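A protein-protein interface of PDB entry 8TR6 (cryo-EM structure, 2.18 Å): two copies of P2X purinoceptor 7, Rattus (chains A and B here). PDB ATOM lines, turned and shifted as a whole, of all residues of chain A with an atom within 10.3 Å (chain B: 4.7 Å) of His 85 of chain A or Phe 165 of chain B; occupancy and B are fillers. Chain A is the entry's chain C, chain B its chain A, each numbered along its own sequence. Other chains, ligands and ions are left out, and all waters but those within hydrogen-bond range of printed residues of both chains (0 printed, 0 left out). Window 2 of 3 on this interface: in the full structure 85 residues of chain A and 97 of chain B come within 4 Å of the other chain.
The backbone NH of Ile 87 of chain A lies within hydrogen-bond range of the side-chain amide oxygen of Gln 116 of chain B (2.8 Å).
Of chain B, only Phe 165 comes within 4 Å of His 85 of chain A.
Of the printed residues of chain A, Phe 165 of chain B touches Glu 70 (3.7 Å), His 85 (3.3 Å) and Ile 87 (3.7 Å).
Gly 146 of chain B touches one residue of chain A.
Ile 164 of chain B touches none of the printed residues of chain A.
Printed residues of chain B within 4 Å of Ile 87 of chain A: Gln 116, Ile 147, Phe 165 and Ala 166.
Of the printed residues of chain A, Ile 147 of chain B touches Val 68 (3.7 Å), Glu 70 (3.5 Å) and Ile 87 (3.2 Å).
The nearest printed residue of chain A that does not touch Phe 165 of chain B is Gly 86 of chain A (4.1 Å).
The nearest printed residue of chain B that does not touch Gly 86 of chain A is Phe 165 of chain B (4.1 Å).
The backbone NH (N) of Phe 165 of chain B is in hydrogen-bond range of the backbone carbonyl oxygen (O) of Ile 147 of chain B.
The backbone carbonyl oxygen (O) of Lys 117 of chain B lies within hydrogen-bond range of the backbone NH (N) of Ala 166 of chain B (2.9 Å).
The backbone NH of Gly 86 of chain A lies within hydrogen-bond range of the backbone carbonyl oxygen of Val 71 of chain A, 2.9 Å away.
OE2 of Glu 70 of chain A is in hydrogen-bond range of NE2 of His 85 of chain A (2.5 Å).
No position is printed for both chains.
Of the 10 printed residues of chain B, 5 touch a printed residue of chain A.
Hydrophobic or aromatic side chains of chain B within 4 Å of the printed part of chain A: Ile 147 and Phe 165.
Of the 18 printed residues of chain A, 5 touch a printed residue of chain B.
Hydrophobic or aromatic side chains of chain A that line the printed part of chain B: Val 68, His 85 and Ile 87.
Among the printed residues, merely in contact across the chains: Val 68 of chain A with Gly 146 of chain B (3.9 Å), Val 68 of chain A with Ile 147 of chain B (3.7 Å), Glu 70 of chain A with Ile 147 of chain B (3.5 Å), Glu 70 of chain A with Phe 165 of chain B (3.7 Å), His 85 of chain A with Phe 165 of chain B (3.3 Å), Gly 86 of chain A with Gln 116 of chain B (3.1 Å), Ile 87 of chain A with Ile 147 of chain B (3.2 Å), Ile 87 of chain A with Phe 165 of chain B (3.7 Å) and Ile 87 of chain A with Ala 166 of chain B (3.9 Å).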
ATOM      1  N   GLY A  67     -30.210   2.540   2.058  1.00  0.00           N
ATOM      2  CA  GLY A  67     -28.887   2.461   2.639  1.00  0.00           C
ATOM      3  C   GLY A  67     -28.902   1.871   4.032  1.00  0.00           C
ATOM      4  O   GLY A  67     -29.850   2.008   4.797  1.00  0.00           O
ATOM      5  N   VAL A  68     -27.807   1.201   4.373  1.00  0.00           N
ATOM      6  CA  VAL A  68     -27.624   0.562   5.666  1.00  0.00           C
ATOM      7  C   VAL A  68     -26.242   0.931   6.182  1.00  0.00           C
ATOM      8  O   VAL A  68     -25.270   0.950   5.421  1.00  0.00           O
ATOM      9  CB  VAL A  68     -27.786  -0.970   5.568  1.00  0.00           C
ATOM     10  CG1 VAL A  68     -27.618  -1.610   6.921  1.00  0.00           C
ATOM     11  CG2 VAL A  68     -29.136  -1.325   4.989  1.00  0.00           C
ATOM     12  N   ALA A  69     -26.156   1.228   7.476  1.00  0.00           N
ATOM     13  CA  ALA A  69     -24.905   1.628   8.102  1.00  0.00           C
ATOM     14  C   ALA A  69     -24.621   0.763   9.320  1.00  0.00           C
ATOM     15  O   ALA A  69     -25.535   0.260   9.976  1.00  0.00           O
ATOM     16  CB  ALA A  69     -24.930   3.105   8.510  1.00  0.00           C
ATOM     17  N   GLU A  70     -23.335   0.594   9.608  1.00  0.00           N
ATOM     18  CA  GLU A  70     -22.864  -0.153  10.765  1.00  0.00           C
ATOM     19  C   GLU A  70     -21.998   0.747  11.630  1.00  0.00           C
ATOM     20  O   GLU A  70     -21.133   1.466  11.122  1.00  0.00           O
ATOM     21  CB  GLU A  70     -22.076  -1.391  10.338  1.00  0.00           C
ATOM     22  CG  GLU A  70     -22.661  -2.689  10.843  1.00  0.00           C
ATOM     23  CD  GLU A  70     -21.834  -3.895  10.436  1.00  0.00           C
ATOM     24  OE1 GLU A  70     -21.107  -3.806   9.426  1.00  0.00           O
ATOM     25  OE2 GLU A  70     -21.914  -4.932  11.129  1.00  0.00           O
ATOM     26  N   VAL A  71     -22.240   0.712  12.938  1.00  0.00           N
ATOM     27  CA  VAL A  71     -21.473   1.490  13.901  1.00  0.00           C
ATOM     28  C   VAL A  71     -20.967   0.550  14.982  1.00  0.00           C
ATOM     29  O   VAL A  71     -21.668  -0.383  15.386  1.00  0.00           O
ATOM     30  CB  VAL A  71     -22.312   2.630  14.515  1.00  0.00           C
ATOM     31  CG1 VAL A  71     -21.519   3.355  15.589  1.00  0.00           C
ATOM     32  CG2 VAL A  71     -22.763   3.600  13.437  1.00  0.00           C
ATOM     33  N   THR A  72     -19.738   0.781  15.436  1.00  0.00           N
ATOM     34  CA  THR A  72     -19.154   0.017  16.534  1.00  0.00           C
ATOM     35  C   THR A  72     -18.504   1.018  17.476  1.00  0.00           C
ATOM     36  O   THR A  72     -17.497   1.637  17.123  1.00  0.00           O
ATOM     37  CB  THR A  72     -18.138  -1.009  16.031  1.00  0.00           C
ATOM     38  OG1 THR A  72     -18.789  -1.939  15.158  1.00  0.00           O
ATOM     39  CG2 THR A  72     -17.525  -1.762  17.197  1.00  0.00           C
ATOM     40  N   GLU A  73     -19.076   1.176  18.666  1.00  0.00           N
ATOM     41  CA  GLU A  73     -18.629   2.208  19.595  1.00  0.00           C
ATOM     42  C   GLU A  73     -18.631   1.631  21.006  1.00  0.00           C
ATOM     43  O   GLU A  73     -18.715   0.416  21.200  1.00  0.00           O
ATOM     44  CB  GLU A  73     -19.515   3.456  19.463  1.00  0.00           C
ATOM     45  CG  GLU A  73     -19.237   4.280  18.217  1.00  0.00           C
ATOM     46  CD  GLU A  73     -17.850   4.892  18.215  1.00  0.00           C
ATOM     47  OE1 GLU A  73     -17.549   5.689  19.127  1.00  0.00           O
ATOM     48  OE2 GLU A  73     -17.059   4.577  17.300  1.00  0.00           O
ATOM     49  N   ASN A  74     -18.505   2.509  21.998  1.00  0.00           N
ATOM     50  CA  ASN A  74     -18.511   2.102  23.398  1.00  0.00           C
ATOM     51  C   ASN A  74     -19.523   2.920  24.191  1.00  0.00           C
ATOM     52  O   ASN A  74     -20.116   2.429  25.152  1.00  0.00           O
ATOM     53  CB  ASN A  74     -17.118   2.260  24.006  1.00  0.00           C
ATOM     54  CG  ASN A  74     -16.159   1.174  23.560  1.00  0.00           C
ATOM     55  OD1 ASN A  74     -16.575   0.085  23.169  1.00  0.00           O
ATOM     56  ND2 ASN A  74     -14.867   1.468  23.616  1.00  0.00           N
ATOM     57  N   LYS A  82     -18.878  -0.770  27.521  1.00  0.00           N
ATOM     58  CA  LYS A  82     -18.970  -2.024  26.790  1.00  0.00           C
ATOM     59  C   LYS A  82     -19.090  -1.736  25.302  1.00  0.00           C
ATOM     60  O   LYS A  82     -19.651  -0.716  24.895  1.00  0.00           O
ATOM     61  CB  LYS A  82     -20.169  -2.862  27.259  1.00  0.00           C
ATOM     62  CG  LYS A  82     -21.516  -2.320  26.813  1.00  0.00           C
ATOM     63  CD  LYS A  82     -22.661  -2.968  27.575  1.00  0.00           C
ATOM     64  CE  LYS A  82     -24.009  -2.496  27.057  1.00  0.00           C
ATOM     65  NZ  LYS A  82     -25.136  -2.957  27.915  1.00  0.00           N
ATOM     66  N   LEU A  83     -18.556  -2.646  24.494  1.00  0.00           N
ATOM     67  CA  LEU A  83     -18.616  -2.484  23.048  1.00  0.00           C
ATOM     68  C   LEU A  83     -20.045  -2.682  22.559  1.00  0.00           C
ATOM     69  O   LEU A  83     -20.705  -3.663  22.914  1.00  0.00           O
ATOM     70  CB  LEU A  83     -17.676  -3.471  22.361  1.00  0.00           C
ATOM     71  CG  LEU A  83     -17.401  -3.199  20.881  1.00  0.00           C
ATOM     72  CD1 LEU A  83     -16.449  -2.025  20.716  1.00  0.00           C
ATOM     73  CD2 LEU A  83     -16.845  -4.439  20.202  1.00  0.00           C
ATOM     74  N   VAL A  84     -20.518  -1.746  21.743  1.00  0.00           N
ATOM     75  CA  VAL A  84     -21.868  -1.771  21.193  1.00  0.00           C
ATOM     76  C   VAL A  84     -21.755  -1.802  19.675  1.00  0.00           C
ATOM     77  O   VAL A  84     -21.106  -0.933  19.074  1.00  0.00           O
ATOM     78  CB  VAL A  84     -22.698  -0.566  21.660  1.00  0.00           C
ATOM     79  CG1 VAL A  84     -24.053  -0.555  20.971  1.00  0.00           C
ATOM     80  CG2 VAL A  84     -22.869  -0.598  23.171  1.00  0.00           C
ATOM     81  N   HIS A  85     -22.386  -2.803  19.068  1.00  0.00           N
ATOM     82  CA  HIS A  85     -22.417  -2.998  17.623  1.00  0.00           C
ATOM     83  C   HIS A  85     -23.838  -2.719  17.153  1.00  0.00           C
ATOM     84  O   HIS A  85     -24.750  -3.510  17.417  1.00  0.00           O
ATOM     85  CB  HIS A  85     -21.978  -4.416  17.267  1.00  0.00           C
ATOM     86  CG  HIS A  85     -21.945  -4.693  15.799  1.00  0.00           C
ATOM     87  ND1 HIS A  85     -22.113  -5.958  15.278  1.00  0.00           N
ATOM     88  CD2 HIS A  85     -21.758  -3.873  14.739  1.00  0.00           C
ATOM     89  CE1 HIS A  85     -22.032  -5.904  13.963  1.00  0.00           C
ATOM     90  NE2 HIS A  85     -21.817  -4.649  13.610  1.00  0.00           N
ATOM     91  N   GLY A  86     -24.025  -1.601  16.459  1.00  0.00           N
ATOM     92  CA  GLY A  86     -25.343  -1.146  16.070  1.00  0.00           C
ATOM     93  C   GLY A  86     -25.528  -1.106  14.567  1.00  0.00           C
ATOM     94  O   GLY A  86     -24.595  -0.821  13.812  1.00  0.00           O
ATOM     95  N   ILE A  87     -26.764  -1.425  14.179  1.00  0.00           N
ATOM     96  CA  ILE A  87     -27.125  -1.376  12.727  1.00  0.00           C
ATOM     97  C   ILE A  87     -28.132  -0.201  12.558  1.00  0.00           C
ATOM     98  O   ILE A  87     -29.010   0.044  13.406  1.00  0.00           O
ATOM     99  CB  ILE A  87     -27.754  -2.701  12.282  1.00  0.00           C
ATOM    100  CG1 ILE A  87     -28.191  -2.646  10.819  1.00  0.00           C
ATOM    101  CG2 ILE A  87     -28.953  -3.060  13.151  1.00  0.00           C
ATOM    102  CD1 ILE A  87     -27.047  -2.459   9.852  1.00  0.00           C
ATOM    103  N   PHE A  88     -27.913   0.608  11.549  1.00  0.00           N
ATOM    104  CA  PHE A  88     -28.759   1.760  11.260  1.00  0.00           C
ATOM    105  C   PHE A  88     -29.384   1.575   9.885  1.00  0.00           C
ATOM    106  O   PHE A  88     -28.681   1.597   8.870  1.00  0.00           O
ATOM    107  CB  PHE A  88     -27.954   3.058  11.320  1.00  0.00           C
ATOM    108  CG  PHE A  88     -27.569   3.467  12.709  1.00  0.00           C
ATOM    109  CD1 PHE A  88     -26.483   2.887  13.341  1.00  0.00           C
ATOM    110  CD2 PHE A  88     -28.290   4.433  13.382  1.00  0.00           C
ATOM    111  CE1 PHE A  88     -26.130   3.260  14.615  1.00  0.00           C
ATOM    112  CE2 PHE A  88     -27.938   4.811  14.658  1.00  0.00           C
ATOM    113  CZ  PHE A  88     -26.858   4.225  15.275  1.00  0.00           C
ATOM    114  N   ASP A  89     -30.697   1.388   9.855  1.00  0.00           N
ATOM    115  CA  ASP A  89     -31.468   1.382   8.622  1.00  0.00           C
ATOM    116  C   ASP A  89     -32.267   2.679   8.532  1.00  0.00           C
ATOM    117  O   ASP A  89     -32.162   3.563   9.388  1.00  0.00           O
ATOM    118  CB  ASP A  89     -32.366   0.141   8.537  1.00  0.00           C
ATOM    119  CG  ASP A  89     -33.389   0.060   9.656  1.00  0.00           C
ATOM    120  OD1 ASP A  89     -34.002   1.089  10.003  1.00  0.00           O
ATOM    121  OD2 ASP A  89     -33.593  -1.054  10.180  1.00  0.00           O
ATOM    122  N   ASP A  92     -33.769   4.270  11.371  1.00  0.00           N
ATOM    123  CA  ASP A  92     -32.837   4.700  12.403  1.00  0.00           C
ATOM    124  C   ASP A  92     -32.142   6.020  12.088  1.00  0.00           C
ATOM    125  O   ASP A  92     -31.624   6.657  13.010  1.00  0.00           O
ATOM    126  CB  ASP A  92     -31.770   3.623  12.639  1.00  0.00           C
ATOM    127  CG  ASP A  92     -32.367   2.267  12.960  1.00  0.00           C
ATOM    128  OD1 ASP A  92     -33.236   2.192  13.851  1.00  0.00           O
ATOM    129  OD2 ASP A  92     -31.963   1.274  12.322  1.00  0.00           O
ATOM    130  N   TYR A 108     -23.968  11.299  15.753  1.00  0.00           N
ATOM    131  CA  TYR A 108     -24.879  11.455  16.874  1.00  0.00           C
ATOM    132  C   TYR A 108     -24.109  11.470  18.183  1.00  0.00           C
ATOM    133  O   TYR A 108     -23.048  10.856  18.313  1.00  0.00           O
ATOM    134  CB  TYR A 108     -25.937  10.344  16.901  1.00  0.00           C
ATOM    135  CG  TYR A 108     -25.387   8.954  17.091  1.00  0.00           C
ATOM    136  CD1 TYR A 108     -25.131   8.452  18.358  1.00  0.00           C
ATOM    137  CD2 TYR A 108     -25.138   8.133  16.002  1.00  0.00           C
ATOM    138  CE1 TYR A 108     -24.634   7.183  18.533  1.00  0.00           C
ATOM    139  CE2 TYR A 108     -24.643   6.861  16.168  1.00  0.00           C
ATOM    140  CZ  TYR A 108     -24.393   6.390  17.436  1.00  0.00           C
ATOM    141  OH  TYR A 108     -23.897   5.119  17.601  1.00  0.00           O
ATOM    142  N   GLN B 116     -30.949  -5.996  17.532  1.00  0.00           N
ATOM    143  CA  GLN B 116     -29.833  -5.899  16.594  1.00  0.00           C
ATOM    144  C   GLN B 116     -29.000  -7.165  16.723  1.00  0.00           C
ATOM    145  O   GLN B 116     -28.211  -7.314  17.658  1.00  0.00           O
ATOM    146  CB  GLN B 116     -29.009  -4.648  16.863  1.00  0.00           C
ATOM    147  CG  GLN B 116     -29.813  -3.369  16.753  1.00  0.00           C
ATOM    148  CD  GLN B 116     -29.065  -2.153  17.247  1.00  0.00           C
ATOM    149  OE1 GLN B 116     -28.375  -1.483  16.484  1.00  0.00           O
ATOM    150  NE2 GLN B 116     -29.207  -1.857  18.531  1.00  0.00           N
ATOM    151  N   LYS B 117     -29.179  -8.086  15.782  1.00  0.00           N
ATOM    152  CA  LYS B 117     -28.515  -9.383  15.839  1.00  0.00           C
ATOM    153  C   LYS B 117     -28.580 -10.021  14.456  1.00  0.00           C
ATOM    154  O   LYS B 117     -28.978  -9.383  13.477  1.00  0.00           O
ATOM    155  CB  LYS B 117     -29.155 -10.270  16.912  1.00  0.00           C
ATOM    156  CG  LYS B 117     -30.519 -10.808  16.536  1.00  0.00           C
ATOM    157  CD  LYS B 117     -31.198 -11.469  17.715  1.00  0.00           C
ATOM    158  CE  LYS B 117     -32.663 -11.732  17.429  1.00  0.00           C
ATOM    159  NZ  LYS B 117     -33.253 -12.711  18.375  1.00  0.00           N
ATOM    160  N   LEU B 118     -28.194 -11.290  14.378  1.00  0.00           N
ATOM    161  CA  LEU B 118     -28.179 -12.022  13.120  1.00  0.00           C
ATOM    162  C   LEU B 118     -29.501 -12.749  12.919  1.00  0.00           C
ATOM    163  O   LEU B 118     -30.089 -13.268  13.871  1.00  0.00           O
ATOM    164  CB  LEU B 118     -27.026 -13.024  13.095  1.00  0.00           C
ATOM    165  CG  LEU B 118     -25.675 -12.499  13.575  1.00  0.00           C
ATOM    166  CD1 LEU B 118     -24.700 -13.645  13.758  1.00  0.00           C
ATOM    167  CD2 LEU B 118     -25.131 -11.475  12.604  1.00  0.00           C
ATOM    168  N   GLY B 146     -29.931  -4.979   6.026  1.00  0.00           N
ATOM    169  CA  GLY B 146     -28.976  -5.620   6.904  1.00  0.00           C
ATOM    170  C   GLY B 146     -27.672  -5.845   6.173  1.00  0.00           C
ATOM    171  O   GLY B 146     -27.565  -5.626   4.964  1.00  0.00           O
ATOM    172  N   ILE B 147     -26.671  -6.288   6.926  1.00  0.00           N
ATOM    173  CA  ILE B 147     -25.355  -6.600   6.387  1.00  0.00           C
ATOM    174  C   ILE B 147     -25.192  -8.111   6.388  1.00  0.00           C
ATOM    175  O   ILE B 147     -25.286  -8.757   7.439  1.00  0.00           O
ATOM    176  CB  ILE B 147     -24.233  -5.915   7.178  1.00  0.00           C
ATOM    177  CG1 ILE B 147     -24.241  -4.416   6.885  1.00  0.00           C
ATOM    178  CG2 ILE B 147     -22.882  -6.513   6.823  1.00  0.00           C
ATOM    179  CD1 ILE B 147     -24.643  -3.581   8.041  1.00  0.00           C
ATOM    180  N   THR B 149     -23.724 -11.791   6.385  1.00  0.00           N
ATOM    181  CA  THR B 149     -22.608 -12.476   7.019  1.00  0.00           C
ATOM    182  C   THR B 149     -21.889 -13.429   6.074  1.00  0.00           C
ATOM    183  O   THR B 149     -20.837 -13.964   6.441  1.00  0.00           O
ATOM    184  CB  THR B 149     -23.094 -13.258   8.243  1.00  0.00           C
ATOM    185  OG1 THR B 149     -23.734 -14.466   7.818  1.00  0.00           O
ATOM    186  CG2 THR B 149     -24.075 -12.429   9.058  1.00  0.00           C
ATOM    187  N   GLU B 163     -27.899 -15.147   6.127  1.00  0.00           N
ATOM    188  CA  GLU B 163     -27.894 -14.469   7.411  1.00  0.00           C
ATOM    189  C   GLU B 163     -27.426 -13.029   7.248  1.00  0.00           C
ATOM    190  O   GLU B 163     -26.476 -12.746   6.512  1.00  0.00           O
ATOM    191  CB  GLU B 163     -26.983 -15.210   8.388  1.00  0.00           C
ATOM    192  CG  GLU B 163     -27.011 -14.684   9.805  1.00  0.00           C
ATOM    193  CD  GLU B 163     -26.183 -15.530  10.750  1.00  0.00           C
ATOM    194  OE1 GLU B 163     -24.939 -15.442  10.690  1.00  0.00           O
ATOM    195  OE2 GLU B 163     -26.775 -16.282  11.553  1.00  0.00           O
ATOM    196  N   ILE B 164     -28.104 -12.120   7.938  1.00  0.00           N
ATOM    197  CA  ILE B 164     -27.776 -10.702   7.921  1.00  0.00           C
ATOM    198  C   ILE B 164     -27.786 -10.195   9.354  1.00  0.00           C
ATOM    199  O   ILE B 164     -28.603 -10.632  10.174  1.00  0.00           O
ATOM    200  CB  ILE B 164     -28.766  -9.890   7.059  1.00  0.00           C
ATOM    201  CG1 ILE B 164     -30.209 -10.269   7.398  1.00  0.00           C
ATOM    202  CG2 ILE B 164     -28.490 -10.106   5.582  1.00  0.00           C
ATOM    203  CD1 ILE B 164     -31.226  -9.228   7.006  1.00  0.00           C
ATOM    204  N   PHE B 165     -26.856  -9.293   9.658  1.00  0.00           N
ATOM    205  CA  PHE B 165     -26.881  -8.559  10.916  1.00  0.00           C
ATOM    206  C   PHE B 165     -27.806  -7.366  10.728  1.00  0.00           C
ATOM    207  O   PHE B 165     -27.496  -6.442   9.969  1.00  0.00           O
ATOM    208  CB  PHE B 165     -25.483  -8.110  11.325  1.00  0.00           C
ATOM    209  CG  PHE B 165     -25.468  -7.228  12.539  1.00  0.00           C
ATOM    210  CD1 PHE B 165     -25.717  -7.755  13.793  1.00  0.00           C
ATOM    211  CD2 PHE B 165     -25.215  -5.874  12.426  1.00  0.00           C
ATOM    212  CE1 PHE B 165     -25.710  -6.948  14.911  1.00  0.00           C
ATOM    213  CE2 PHE B 165     -25.205  -5.064  13.544  1.00  0.00           C
ATOM    214  CZ  PHE B 165     -25.455  -5.603  14.786  1.00  0.00           C
ATOM    215  N   ALA B 166     -28.944  -7.386  11.407  1.00  0.00           N
ATOM    216  CA  ALA B 166     -29.964  -6.367  11.230  1.00  0.00           C
ATOM    217  C   ALA B 166     -30.883  -6.388  12.443  1.00  0.00           C
ATOM    218  O   ALA B 166     -30.614  -7.067  13.441  1.00  0.00           O
ATOM    219  CB  ALA B 166     -30.744  -6.605   9.933  1.00  0.00           C
